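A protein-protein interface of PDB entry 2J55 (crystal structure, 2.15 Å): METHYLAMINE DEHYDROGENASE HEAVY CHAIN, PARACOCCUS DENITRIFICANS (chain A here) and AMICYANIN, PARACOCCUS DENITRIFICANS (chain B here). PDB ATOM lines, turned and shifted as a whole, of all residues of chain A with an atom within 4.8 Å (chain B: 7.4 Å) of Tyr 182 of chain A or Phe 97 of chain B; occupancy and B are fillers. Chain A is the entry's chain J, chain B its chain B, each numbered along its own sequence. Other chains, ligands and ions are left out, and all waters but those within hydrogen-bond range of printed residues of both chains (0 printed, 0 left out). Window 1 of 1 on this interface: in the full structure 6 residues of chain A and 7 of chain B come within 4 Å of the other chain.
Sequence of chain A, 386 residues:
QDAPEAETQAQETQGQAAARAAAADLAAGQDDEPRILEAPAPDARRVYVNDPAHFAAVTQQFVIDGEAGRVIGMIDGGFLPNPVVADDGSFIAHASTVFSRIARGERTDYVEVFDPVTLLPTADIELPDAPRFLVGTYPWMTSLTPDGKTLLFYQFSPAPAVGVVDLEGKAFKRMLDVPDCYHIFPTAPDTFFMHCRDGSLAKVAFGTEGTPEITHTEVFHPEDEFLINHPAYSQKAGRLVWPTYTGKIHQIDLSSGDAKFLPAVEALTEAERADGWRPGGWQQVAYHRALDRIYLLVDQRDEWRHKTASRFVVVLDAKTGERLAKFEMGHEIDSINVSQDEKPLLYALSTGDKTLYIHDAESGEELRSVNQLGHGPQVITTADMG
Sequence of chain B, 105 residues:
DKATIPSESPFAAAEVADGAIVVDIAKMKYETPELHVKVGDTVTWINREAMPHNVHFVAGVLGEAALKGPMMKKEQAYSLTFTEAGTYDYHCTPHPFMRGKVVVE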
ATOM      1  N   MET A 141      -4.830  -2.943 -34.324  1.00  0.00           N
ATOM      2  CA  MET A 141      -5.573  -2.473 -33.124  1.00  0.00           C
ATOM      3  C   MET A 141      -5.345  -0.984 -32.878  1.00  0.00           C
ATOM      4  O   MET A 141      -6.059  -0.359 -32.083  1.00  0.00           O
ATOM      5  CB  MET A 141      -5.262  -3.304 -31.898  1.00  0.00           C
ATOM      6  CG  MET A 141      -5.963  -4.620 -31.885  1.00  0.00           C
ATOM      7  SD  MET A 141      -7.702  -4.411 -31.569  1.00  0.00           S
ATOM      8  CE  MET A 141      -8.302  -6.100 -31.733  1.00  0.00           C
ATOM      9  N   TYR A 154      -8.064   0.922 -30.450  1.00  0.00           N
ATOM     10  CA  TYR A 154      -9.173   0.125 -29.914  1.00  0.00           C
ATOM     11  C   TYR A 154      -9.209   0.067 -28.360  1.00  0.00           C
ATOM     12  O   TYR A 154      -8.189  -0.030 -27.716  1.00  0.00           O
ATOM     13  CB  TYR A 154      -9.136  -1.280 -30.528  1.00  0.00           C
ATOM     14  CG  TYR A 154     -10.299  -2.155 -30.083  1.00  0.00           C
ATOM     15  CD1 TYR A 154     -11.608  -1.941 -30.590  1.00  0.00           C
ATOM     16  CD2 TYR A 154     -10.107  -3.203 -29.170  1.00  0.00           C
ATOM     17  CE1 TYR A 154     -12.676  -2.743 -30.176  1.00  0.00           C
ATOM     18  CE2 TYR A 154     -11.187  -4.039 -28.762  1.00  0.00           C
ATOM     19  CZ  TYR A 154     -12.480  -3.789 -29.289  1.00  0.00           C
ATOM     20  OH  TYR A 154     -13.567  -4.514 -28.880  1.00  0.00           O
ATOM     21  N   PHE A 156     -11.214  -2.132 -25.413  1.00  0.00           N
ATOM     22  CA  PHE A 156     -11.987  -3.349 -25.233  1.00  0.00           C
ATOM     23  C   PHE A 156     -12.940  -3.231 -24.064  1.00  0.00           C
ATOM     24  O   PHE A 156     -14.127  -3.612 -24.180  1.00  0.00           O
ATOM     25  CB  PHE A 156     -11.009  -4.514 -25.108  1.00  0.00           C
ATOM     26  CG  PHE A 156     -11.606  -5.787 -24.676  1.00  0.00           C
ATOM     27  CD1 PHE A 156     -12.238  -6.650 -25.624  1.00  0.00           C
ATOM     28  CD2 PHE A 156     -11.470  -6.196 -23.331  1.00  0.00           C
ATOM     29  CE1 PHE A 156     -12.825  -7.880 -25.252  1.00  0.00           C
ATOM     30  CE2 PHE A 156     -12.023  -7.439 -22.921  1.00  0.00           C
ATOM     31  CZ  PHE A 156     -12.741  -8.298 -23.912  1.00  0.00           C
ATOM     32  N   ASP A 180     -19.963  -4.615 -30.857  1.00  0.00           N
ATOM     33  CA  ASP A 180     -19.109  -5.802 -30.555  1.00  0.00           C
ATOM     34  C   ASP A 180     -18.245  -6.261 -31.737  1.00  0.00           C
ATOM     35  O   ASP A 180     -18.345  -7.428 -32.180  1.00  0.00           O
ATOM     36  CB  ASP A 180     -19.936  -6.974 -29.982  1.00  0.00           C
ATOM     37  CG  ASP A 180     -19.075  -8.230 -29.612  1.00  0.00           C
ATOM     38  OD1 ASP A 180     -17.815  -8.205 -29.597  1.00  0.00           O
ATOM     39  OD2 ASP A 180     -19.679  -9.278 -29.320  1.00  0.00           O
ATOM     40  N   CYS A 181     -17.369  -5.342 -32.219  1.00  0.00           N
ATOM     41  CA  CYS A 181     -16.321  -5.585 -33.224  1.00  0.00           C
ATOM     42  C   CYS A 181     -14.878  -5.235 -32.748  1.00  0.00           C
ATOM     43  O   CYS A 181     -14.657  -4.771 -31.599  1.00  0.00           O
ATOM     44  CB  CYS A 181     -16.611  -4.824 -34.533  1.00  0.00           C
ATOM     45  SG  CYS A 181     -18.400  -4.771 -34.963  1.00  0.00           S
ATOM     46  N   TYR A 182     -13.905  -5.465 -33.639  1.00  0.00           N
ATOM     47  CA  TYR A 182     -12.502  -5.619 -33.267  1.00  0.00           C
ATOM     48  C   TYR A 182     -11.654  -5.310 -34.419  1.00  0.00           C
ATOM     49  O   TYR A 182     -11.995  -5.772 -35.515  1.00  0.00           O
ATOM     50  CB  TYR A 182     -12.219  -7.068 -32.923  1.00  0.00           C
ATOM     51  CG  TYR A 182     -12.981  -7.455 -31.734  1.00  0.00           C
ATOM     52  CD1 TYR A 182     -14.280  -7.942 -31.862  1.00  0.00           C
ATOM     53  CD2 TYR A 182     -12.435  -7.289 -30.439  1.00  0.00           C
ATOM     54  CE1 TYR A 182     -15.049  -8.251 -30.768  1.00  0.00           C
ATOM     55  CE2 TYR A 182     -13.188  -7.671 -29.330  1.00  0.00           C
ATOM     56  CZ  TYR A 182     -14.505  -8.123 -29.504  1.00  0.00           C
ATOM     57  OH  TYR A 182     -15.298  -8.466 -28.430  1.00  0.00           O
ATOM     58  N   HIS A 183     -10.558  -4.573 -34.175  1.00  0.00           N
ATOM     59  CA  HIS A 183      -9.557  -4.216 -35.192  1.00  0.00           C
ATOM     60  C   HIS A 183      -9.942  -2.952 -36.007  1.00  0.00           C
ATOM     61  O   HIS A 183     -11.103  -2.581 -36.113  1.00  0.00           O
ATOM     62  CB  HIS A 183      -9.345  -5.365 -36.165  1.00  0.00           C
ATOM     63  CG  HIS A 183      -8.396  -6.442 -35.709  1.00  0.00           C
ATOM     64  ND1 HIS A 183      -8.830  -7.654 -35.211  1.00  0.00           N
ATOM     65  CD2 HIS A 183      -7.054  -6.550 -35.835  1.00  0.00           C
ATOM     66  CE1 HIS A 183      -7.788  -8.442 -35.008  1.00  0.00           C
ATOM     67  NE2 HIS A 183      -6.700  -7.801 -35.387  1.00  0.00           N
ATOM     68  N   ILE A 184      -8.956  -2.267 -36.550  1.00  0.00           N
ATOM     69  CA  ILE A 184      -9.221  -0.960 -37.113  1.00  0.00           C
ATOM     70  C   ILE A 184      -8.502  -0.797 -38.431  1.00  0.00           C
ATOM     71  O   ILE A 184      -7.283  -0.627 -38.445  1.00  0.00           O
ATOM     72  CB  ILE A 184      -8.849   0.209 -36.172  1.00  0.00           C
ATOM     73  CG1 ILE A 184      -9.639   0.163 -34.848  1.00  0.00           C
ATOM     74  CG2 ILE A 184      -9.077   1.531 -36.864  1.00  0.00           C
ATOM     75  CD1 ILE A 184      -9.028   1.040 -33.724  1.00  0.00           C
ATOM     76  N   PHE A 185      -9.286  -0.834 -39.532  1.00  0.00           N
ATOM     77  CA  PHE A 185      -8.764  -0.756 -40.889  1.00  0.00           C
ATOM     78  C   PHE A 185      -9.343   0.557 -41.502  1.00  0.00           C
ATOM     79  O   PHE A 185     -10.529   0.617 -41.927  1.00  0.00           O
ATOM     80  CB  PHE A 185      -9.168  -1.992 -41.734  1.00  0.00           C
ATOM     81  CG  PHE A 185      -9.062  -3.316 -41.018  1.00  0.00           C
ATOM     82  CD1 PHE A 185      -7.835  -4.000 -40.955  1.00  0.00           C
ATOM     83  CD2 PHE A 185     -10.196  -3.896 -40.454  1.00  0.00           C
ATOM     84  CE1 PHE A 185      -7.706  -5.254 -40.330  1.00  0.00           C
ATOM     85  CE2 PHE A 185     -10.115  -5.100 -39.794  1.00  0.00           C
ATOM     86  CZ  PHE A 185      -8.825  -5.813 -39.730  1.00  0.00           C
ATOM     87  N   MET A 194     -14.105  -2.450 -39.064  1.00  0.00           N
ATOM     88  CA  MET A 194     -13.797  -3.386 -37.995  1.00  0.00           C
ATOM     89  C   MET A 194     -14.482  -4.715 -38.331  1.00  0.00           C
ATOM     90  O   MET A 194     -15.415  -4.721 -39.150  1.00  0.00           O
ATOM     91  CB  MET A 194     -14.394  -2.864 -36.692  1.00  0.00           C
ATOM     92  CG  MET A 194     -14.096  -1.407 -36.429  1.00  0.00           C
ATOM     93  SD  MET A 194     -14.860  -0.889 -34.884  1.00  0.00           S
ATOM     94  CE  MET A 194     -13.715  -1.631 -33.676  1.00  0.00           C
ATOM     95  N   HIS A 195     -14.073  -5.809 -37.658  1.00  0.00           N
ATOM     96  CA  HIS A 195     -14.685  -7.130 -37.782  1.00  0.00           C
ATOM     97  C   HIS A 195     -15.483  -7.612 -36.536  1.00  0.00           C
ATOM     98  O   HIS A 195     -15.040  -7.419 -35.354  1.00  0.00           O
ATOM     99  CB  HIS A 195     -13.606  -8.109 -38.187  1.00  0.00           C
ATOM    100  CG  HIS A 195     -14.012  -9.541 -38.076  1.00  0.00           C
ATOM    101  ND1 HIS A 195     -13.262 -10.474 -37.396  1.00  0.00           N
ATOM    102  CD2 HIS A 195     -15.106 -10.197 -38.537  1.00  0.00           C
ATOM    103  CE1 HIS A 195     -13.884 -11.639 -37.432  1.00  0.00           C
ATOM    104  NE2 HIS A 195     -15.003 -11.499 -38.125  1.00  0.00           N
ATOM    105  N   ARG A 197     -18.125  -9.931 -33.831  1.00  0.00           N
ATOM    106  CA  ARG A 197     -18.403 -11.236 -33.235  1.00  0.00           C
ATOM    107  C   ARG A 197     -19.428 -11.996 -34.100  1.00  0.00           C
ATOM    108  O   ARG A 197     -19.216 -13.179 -34.416  1.00  0.00           O
ATOM    109  CB  ARG A 197     -18.906 -11.185 -31.799  1.00  0.00           C
ATOM    110  CG  ARG A 197     -19.261 -12.556 -31.344  1.00  0.00           C
ATOM    111  CD  ARG A 197     -20.070 -12.610 -30.157  1.00  0.00           C
ATOM    112  NE  ARG A 197     -19.074 -12.868 -29.180  1.00  0.00           N
ATOM    113  CZ  ARG A 197     -18.951 -13.895 -28.366  1.00  0.00           C
ATOM    114  NH1 ARG A 197     -17.893 -13.846 -27.598  1.00  0.00           N
ATOM    115  NH2 ARG A 197     -19.843 -14.863 -28.222  1.00  0.00           N
ATOM    116  N   LYS B  27     -25.636 -18.725 -24.027  1.00  0.00           N
ATOM    117  CA  LYS B  27     -25.106 -18.468 -25.348  1.00  0.00           C
ATOM    118  C   LYS B  27     -24.438 -17.071 -25.502  1.00  0.00           C
ATOM    119  O   LYS B  27     -24.507 -16.424 -26.549  1.00  0.00           O
ATOM    120  CB  LYS B  27     -26.144 -18.858 -26.446  1.00  0.00           C
ATOM    121  CG  LYS B  27     -26.479 -20.449 -26.467  1.00  0.00           C
ATOM    122  CD  LYS B  27     -27.706 -20.808 -25.522  1.00  0.00           C
ATOM    123  CE  LYS B  27     -28.527 -22.105 -25.889  1.00  0.00           C
ATOM    124  NZ  LYS B  27     -29.430 -21.985 -27.139  1.00  0.00           N
ATOM    125  N   MET B  28     -23.742 -16.648 -24.440  1.00  0.00           N
ATOM    126  CA  MET B  28     -23.050 -15.356 -24.373  1.00  0.00           C
ATOM    127  C   MET B  28     -23.930 -14.123 -24.412  1.00  0.00           C
ATOM    128  O   MET B  28     -23.502 -13.105 -24.895  1.00  0.00           O
ATOM    129  CB  MET B  28     -22.004 -15.292 -25.456  1.00  0.00           C
ATOM    130  CG  MET B  28     -21.038 -16.530 -25.433  1.00  0.00           C
ATOM    131  SD  MET B  28     -20.065 -16.690 -23.884  1.00  0.00           S
ATOM    132  CE  MET B  28     -19.227 -15.104 -24.004  1.00  0.00           C
ATOM    133  N   LYS B  29     -25.149 -14.223 -23.867  1.00  0.00           N
ATOM    134  CA  LYS B  29     -26.146 -13.164 -23.893  1.00  0.00           C
ATOM    135  C   LYS B  29     -26.956 -13.156 -22.594  1.00  0.00           C
ATOM    136  O   LYS B  29     -27.367 -14.215 -22.060  1.00  0.00           O
ATOM    137  CB  LYS B  29     -27.130 -13.328 -25.133  1.00  0.00           C
ATOM    138  CG  LYS B  29     -26.384 -13.567 -26.499  1.00  0.00           C
ATOM    139  CD  LYS B  29     -27.249 -14.264 -27.702  1.00  0.00           C
ATOM    140  CE  LYS B  29     -27.508 -13.237 -28.836  1.00  0.00           C
ATOM    141  NZ  LYS B  29     -28.073 -13.810 -30.170  1.00  0.00           N
ATOM    142  N   TYR B  30     -27.181 -11.946 -22.102  1.00  0.00           N
ATOM    143  CA  TYR B  30     -28.285 -11.708 -21.210  1.00  0.00           C
ATOM    144  C   TYR B  30     -29.617 -11.905 -21.959  1.00  0.00           C
ATOM    145  O   TYR B  30     -29.757 -11.472 -23.093  1.00  0.00           O
ATOM    146  CB  TYR B  30     -28.232 -10.300 -20.602  1.00  0.00           C
ATOM    147  CG  TYR B  30     -26.914  -9.992 -19.851  1.00  0.00           C
ATOM    148  CD1 TYR B  30     -26.632 -10.586 -18.613  1.00  0.00           C
ATOM    149  CD2 TYR B  30     -25.967  -9.105 -20.405  1.00  0.00           C
ATOM    150  CE1 TYR B  30     -25.428 -10.307 -17.936  1.00  0.00           C
ATOM    151  CE2 TYR B  30     -24.805  -8.808 -19.759  1.00  0.00           C
ATOM    152  CZ  TYR B  30     -24.523  -9.394 -18.523  1.00  0.00           C
ATOM    153  OH  TYR B  30     -23.345  -9.060 -17.915  1.00  0.00           O
ATOM    154  N   HIS B  53     -19.983 -15.917 -15.817  1.00  0.00           N
ATOM    155  CA  HIS B  53     -20.436 -14.567 -16.211  1.00  0.00           C
ATOM    156  C   HIS B  53     -20.715 -13.749 -15.028  1.00  0.00           C
ATOM    157  O   HIS B  53     -20.978 -14.292 -13.949  1.00  0.00           O
ATOM    158  CB  HIS B  53     -21.763 -14.618 -17.019  1.00  0.00           C
ATOM    159  CG  HIS B  53     -21.694 -15.362 -18.327  1.00  0.00           C
ATOM    160  ND1 HIS B  53     -20.932 -14.942 -19.382  1.00  0.00           N
ATOM    161  CD2 HIS B  53     -22.399 -16.425 -18.786  1.00  0.00           C
ATOM    162  CE1 HIS B  53     -21.126 -15.730 -20.423  1.00  0.00           C
ATOM    163  NE2 HIS B  53     -22.015 -16.636 -20.086  1.00  0.00           N
ATOM    164  N   HIS B  91     -22.454  -4.615 -17.725  1.00  0.00           N
ATOM    165  CA  HIS B  91     -21.762  -5.507 -18.650  1.00  0.00           C
ATOM    166  C   HIS B  91     -21.127  -6.698 -17.898  1.00  0.00           C
ATOM    167  O   HIS B  91     -21.201  -6.793 -16.630  1.00  0.00           O
ATOM    168  CB  HIS B  91     -20.753  -4.779 -19.502  1.00  0.00           C
ATOM    169  CG  HIS B  91     -19.474  -4.422 -18.787  1.00  0.00           C
ATOM    170  ND1 HIS B  91     -19.342  -3.299 -18.012  1.00  0.00           N
ATOM    171  CD2 HIS B  91     -18.253  -5.015 -18.792  1.00  0.00           C
ATOM    172  CE1 HIS B  91     -18.108  -3.222 -17.548  1.00  0.00           C
ATOM    173  NE2 HIS B  91     -17.425  -4.249 -18.013  1.00  0.00           N
ATOM    174  N   CYS B  92     -20.625  -7.634 -18.683  1.00  0.00           N
ATOM    175  CA  CYS B  92     -19.922  -8.783 -18.137  1.00  0.00           C
ATOM    176  C   CYS B  92     -18.409  -8.501 -18.152  1.00  0.00           C
ATOM    177  O   CYS B  92     -17.833  -8.254 -19.185  1.00  0.00           O
ATOM    178  CB  CYS B  92     -20.231 -10.057 -18.928  1.00  0.00           C
ATOM    179  SG  CYS B  92     -19.494 -11.548 -18.081  1.00  0.00           S
ATOM    180  N   THR B  93     -17.782  -8.520 -16.986  1.00  0.00           N
ATOM    181  CA  THR B  93     -16.395  -8.060 -16.849  1.00  0.00           C
ATOM    182  C   THR B  93     -15.438  -8.633 -17.885  1.00  0.00           C
ATOM    183  O   THR B  93     -14.795  -7.875 -18.525  1.00  0.00           O
ATOM    184  CB  THR B  93     -15.906  -8.293 -15.461  1.00  0.00           C
ATOM    185  OG1 THR B  93     -16.749  -7.615 -14.569  1.00  0.00           O
ATOM    186  CG2 THR B  93     -14.478  -7.792 -15.219  1.00  0.00           C
ATOM    187  N   PRO B  94     -15.377  -9.969 -18.087  1.00  0.00           N
ATOM    188  CA  PRO B  94     -14.576 -10.478 -19.198  1.00  0.00           C
ATOM    189  C   PRO B  94     -15.205 -10.314 -20.567  1.00  0.00           C
ATOM    190  O   PRO B  94     -14.496 -10.439 -21.550  1.00  0.00           O
ATOM    191  CB  PRO B  94     -14.518 -11.962 -18.912  1.00  0.00           C
ATOM    192  CG  PRO B  94     -15.755 -12.257 -18.181  1.00  0.00           C
ATOM    193  CD  PRO B  94     -15.963 -11.080 -17.317  1.00  0.00           C
ATOM    194  N   HIS B  95     -16.524 -10.069 -20.657  1.00  0.00           N
ATOM    195  CA  HIS B  95     -17.142 -10.003 -21.979  1.00  0.00           C
ATOM    196  C   HIS B  95     -17.817  -8.655 -22.189  1.00  0.00           C
ATOM    197  O   HIS B  95     -19.029  -8.616 -22.113  1.00  0.00           O
ATOM    198  CB  HIS B  95     -18.213 -11.125 -22.144  1.00  0.00           C
ATOM    199  CG  HIS B  95     -17.843 -12.455 -21.563  1.00  0.00           C
ATOM    200  ND1 HIS B  95     -18.727 -13.212 -20.779  1.00  0.00           N
ATOM    201  CD2 HIS B  95     -16.680 -13.156 -21.648  1.00  0.00           C
ATOM    202  CE1 HIS B  95     -18.071 -14.301 -20.390  1.00  0.00           C
ATOM    203  NE2 HIS B  95     -16.831 -14.275 -20.880  1.00  0.00           N
ATOM    204  N   PRO B  96     -17.066  -7.538 -22.431  1.00  0.00           N
ATOM    205  CA  PRO B  96     -17.724  -6.172 -22.549  1.00  0.00           C
ATOM    206  C   PRO B  96     -18.921  -6.069 -23.516  1.00  0.00           C
ATOM    207  O   PRO B  96     -19.729  -5.138 -23.411  1.00  0.00           O
ATOM    208  CB  PRO B  96     -16.617  -5.301 -23.137  1.00  0.00           C
ATOM    209  CG  PRO B  96     -15.333  -5.953 -22.710  1.00  0.00           C
ATOM    210  CD  PRO B  96     -15.601  -7.445 -22.646  1.00  0.00           C
ATOM    211  N   PHE B  97     -18.924  -6.960 -24.507  1.00  0.00           N
ATOM    212  CA  PHE B  97     -19.976  -7.119 -25.527  1.00  0.00           C
ATOM    213  C   PHE B  97     -21.320  -7.679 -25.007  1.00  0.00           C
ATOM    214  O   PHE B  97     -22.365  -7.607 -25.689  1.00  0.00           O
ATOM    215  CB  PHE B  97     -19.429  -8.019 -26.635  1.00  0.00           C
ATOM    216  CG  PHE B  97     -19.194  -9.458 -26.214  1.00  0.00           C
ATOM    217  CD1 PHE B  97     -20.233 -10.416 -26.303  1.00  0.00           C
ATOM    218  CD2 PHE B  97     -17.922  -9.879 -25.768  1.00  0.00           C
ATOM    219  CE1 PHE B  97     -19.990 -11.757 -25.912  1.00  0.00           C
ATOM    220  CE2 PHE B  97     -17.680 -11.197 -25.374  1.00  0.00           C
ATOM    221  CZ  PHE B  97     -18.684 -12.134 -25.444  1.00  0.00           C
ATOM    222  N   MET B  98     -21.286  -8.284 -23.825  1.00  0.00           N
ATOM    223  CA  MET B  98     -22.459  -8.630 -23.134  1.00  0.00           C
ATOM    224  C   MET B  98     -22.839  -7.369 -22.352  1.00  0.00           C
ATOM    225  O   MET B  98     -22.136  -6.976 -21.418  1.00  0.00           O
ATOM    226  CB  MET B  98     -22.188  -9.818 -22.208  1.00  0.00           C
ATOM    227  CG  MET B  98     -21.838 -11.123 -22.936  1.00  0.00           C
ATOM    228  SD  MET B  98     -21.745 -12.588 -21.851  1.00  0.00           S
ATOM    229  CE  MET B  98     -23.249 -12.659 -20.862  1.00  0.00           C
ATOM    230  N   ARG B  99     -23.953  -6.756 -22.738  1.00  0.00           N
ATOM    231  CA  ARG B  99     -24.444  -5.515 -22.141  1.00  0.00           C
ATOM    232  C   ARG B  99     -25.927  -5.583 -21.764  1.00  0.00           C
ATOM    233  O   ARG B  99     -26.778  -6.140 -22.490  1.00  0.00           O
ATOM    234  CB  ARG B  99     -24.173  -4.313 -23.029  1.00  0.00           C
ATOM    235  CG  ARG B  99     -22.740  -4.110 -23.533  1.00  0.00           C
ATOM    236  CD  ARG B  99     -22.766  -2.865 -24.396  1.00  0.00           C
ATOM    237  NE  ARG B  99     -22.026  -2.908 -25.667  1.00  0.00           N
ATOM    238  CZ  ARG B  99     -22.250  -3.708 -26.718  1.00  0.00           C
ATOM    239  NH1 ARG B  99     -23.184  -4.643 -26.715  1.00  0.00           N
ATOM    240  NH2 ARG B  99     -21.478  -3.601 -27.787  1.00  0.00           N
ATOM    241  N   GLY B 100     -26.265  -4.982 -20.639  1.00  0.00           N
ATOM    242  CA  GLY B 100     -27.672  -4.961 -20.257  1.00  0.00           C
ATOM    243  C   GLY B 100     -28.018  -3.611 -19.693  1.00  0.00           C
ATOM    244  O   GLY B 100     -27.129  -2.808 -19.489  1.00  0.00           O
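Among the printed residues, pairs that only touch across the chains: Arg 197 of chain A with Phe 97 of chain B, Asp 180 of chain A with Phe 97 of chain B, Phe 156 of chain A with Pro 96 of chain B, Arg 197 of chain A with Met 28 of chain B, Asp 180 of chain A with Arg 99 of chain B, Phe 156 of chain A with Pro 94 of chain B and Tyr 182 of chain A with Phe 97 of chain B.
Printed residues of chain B within 4 Å of Tyr 182 of chain A: Phe 97 (3.996 Å).
Of the printed residues of chain A, Phe 97 of chain B touches Asp 180, Tyr 182 and Arg 197.
Of the printed residues of chain B, Asp 180 of chain A touches Phe 97 (3.0 Å) and Arg 99 (3.6 Å).
Printed residues of chain A within 4 Å of Met 28 of chain B: Arg 197.
Met 141 of chain A touches none of the printed residues of chain B.
His 183 of chain A touches none of the printed residues of chain B.
The nearest printed residue of chain B that does not touch Arg 197 of chain A is Lys 27 of chain B (5.2 Å).
OD1 of Asp 180 of chain A is in hydrogen-bond range of OH of Tyr 182 of chain A (2.8 Å).
The side-chain carboxylate (OD2) of Asp 180 of chain A lies within salt-bridge range of the guanidinium group (NE) of Arg 197 of chain A.
The guanidinium group (NH1) of Arg 99 of chain B sits at hydrogen-bond distance from the backbone carbonyl oxygen (O) of Phe 97 of chain B (3.2 Å).
The backbone carbonyl oxygen of His 195 of chain A sits at hydrogen-bond distance from the backbone NH of Tyr 182 of chain A, at 2.8 Å.
Printed residues of chain B that touch a printed residue of chain A: Met 28, Pro 94, Pro 96, Phe 97 and Arg 99.
Among the printed residues, 7 pairs touch across the chains.
Among the printed residues, no Asp or Glu carboxylate lies within 4 Å of a Lys or Arg side-chain nitrogen of the other chain.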
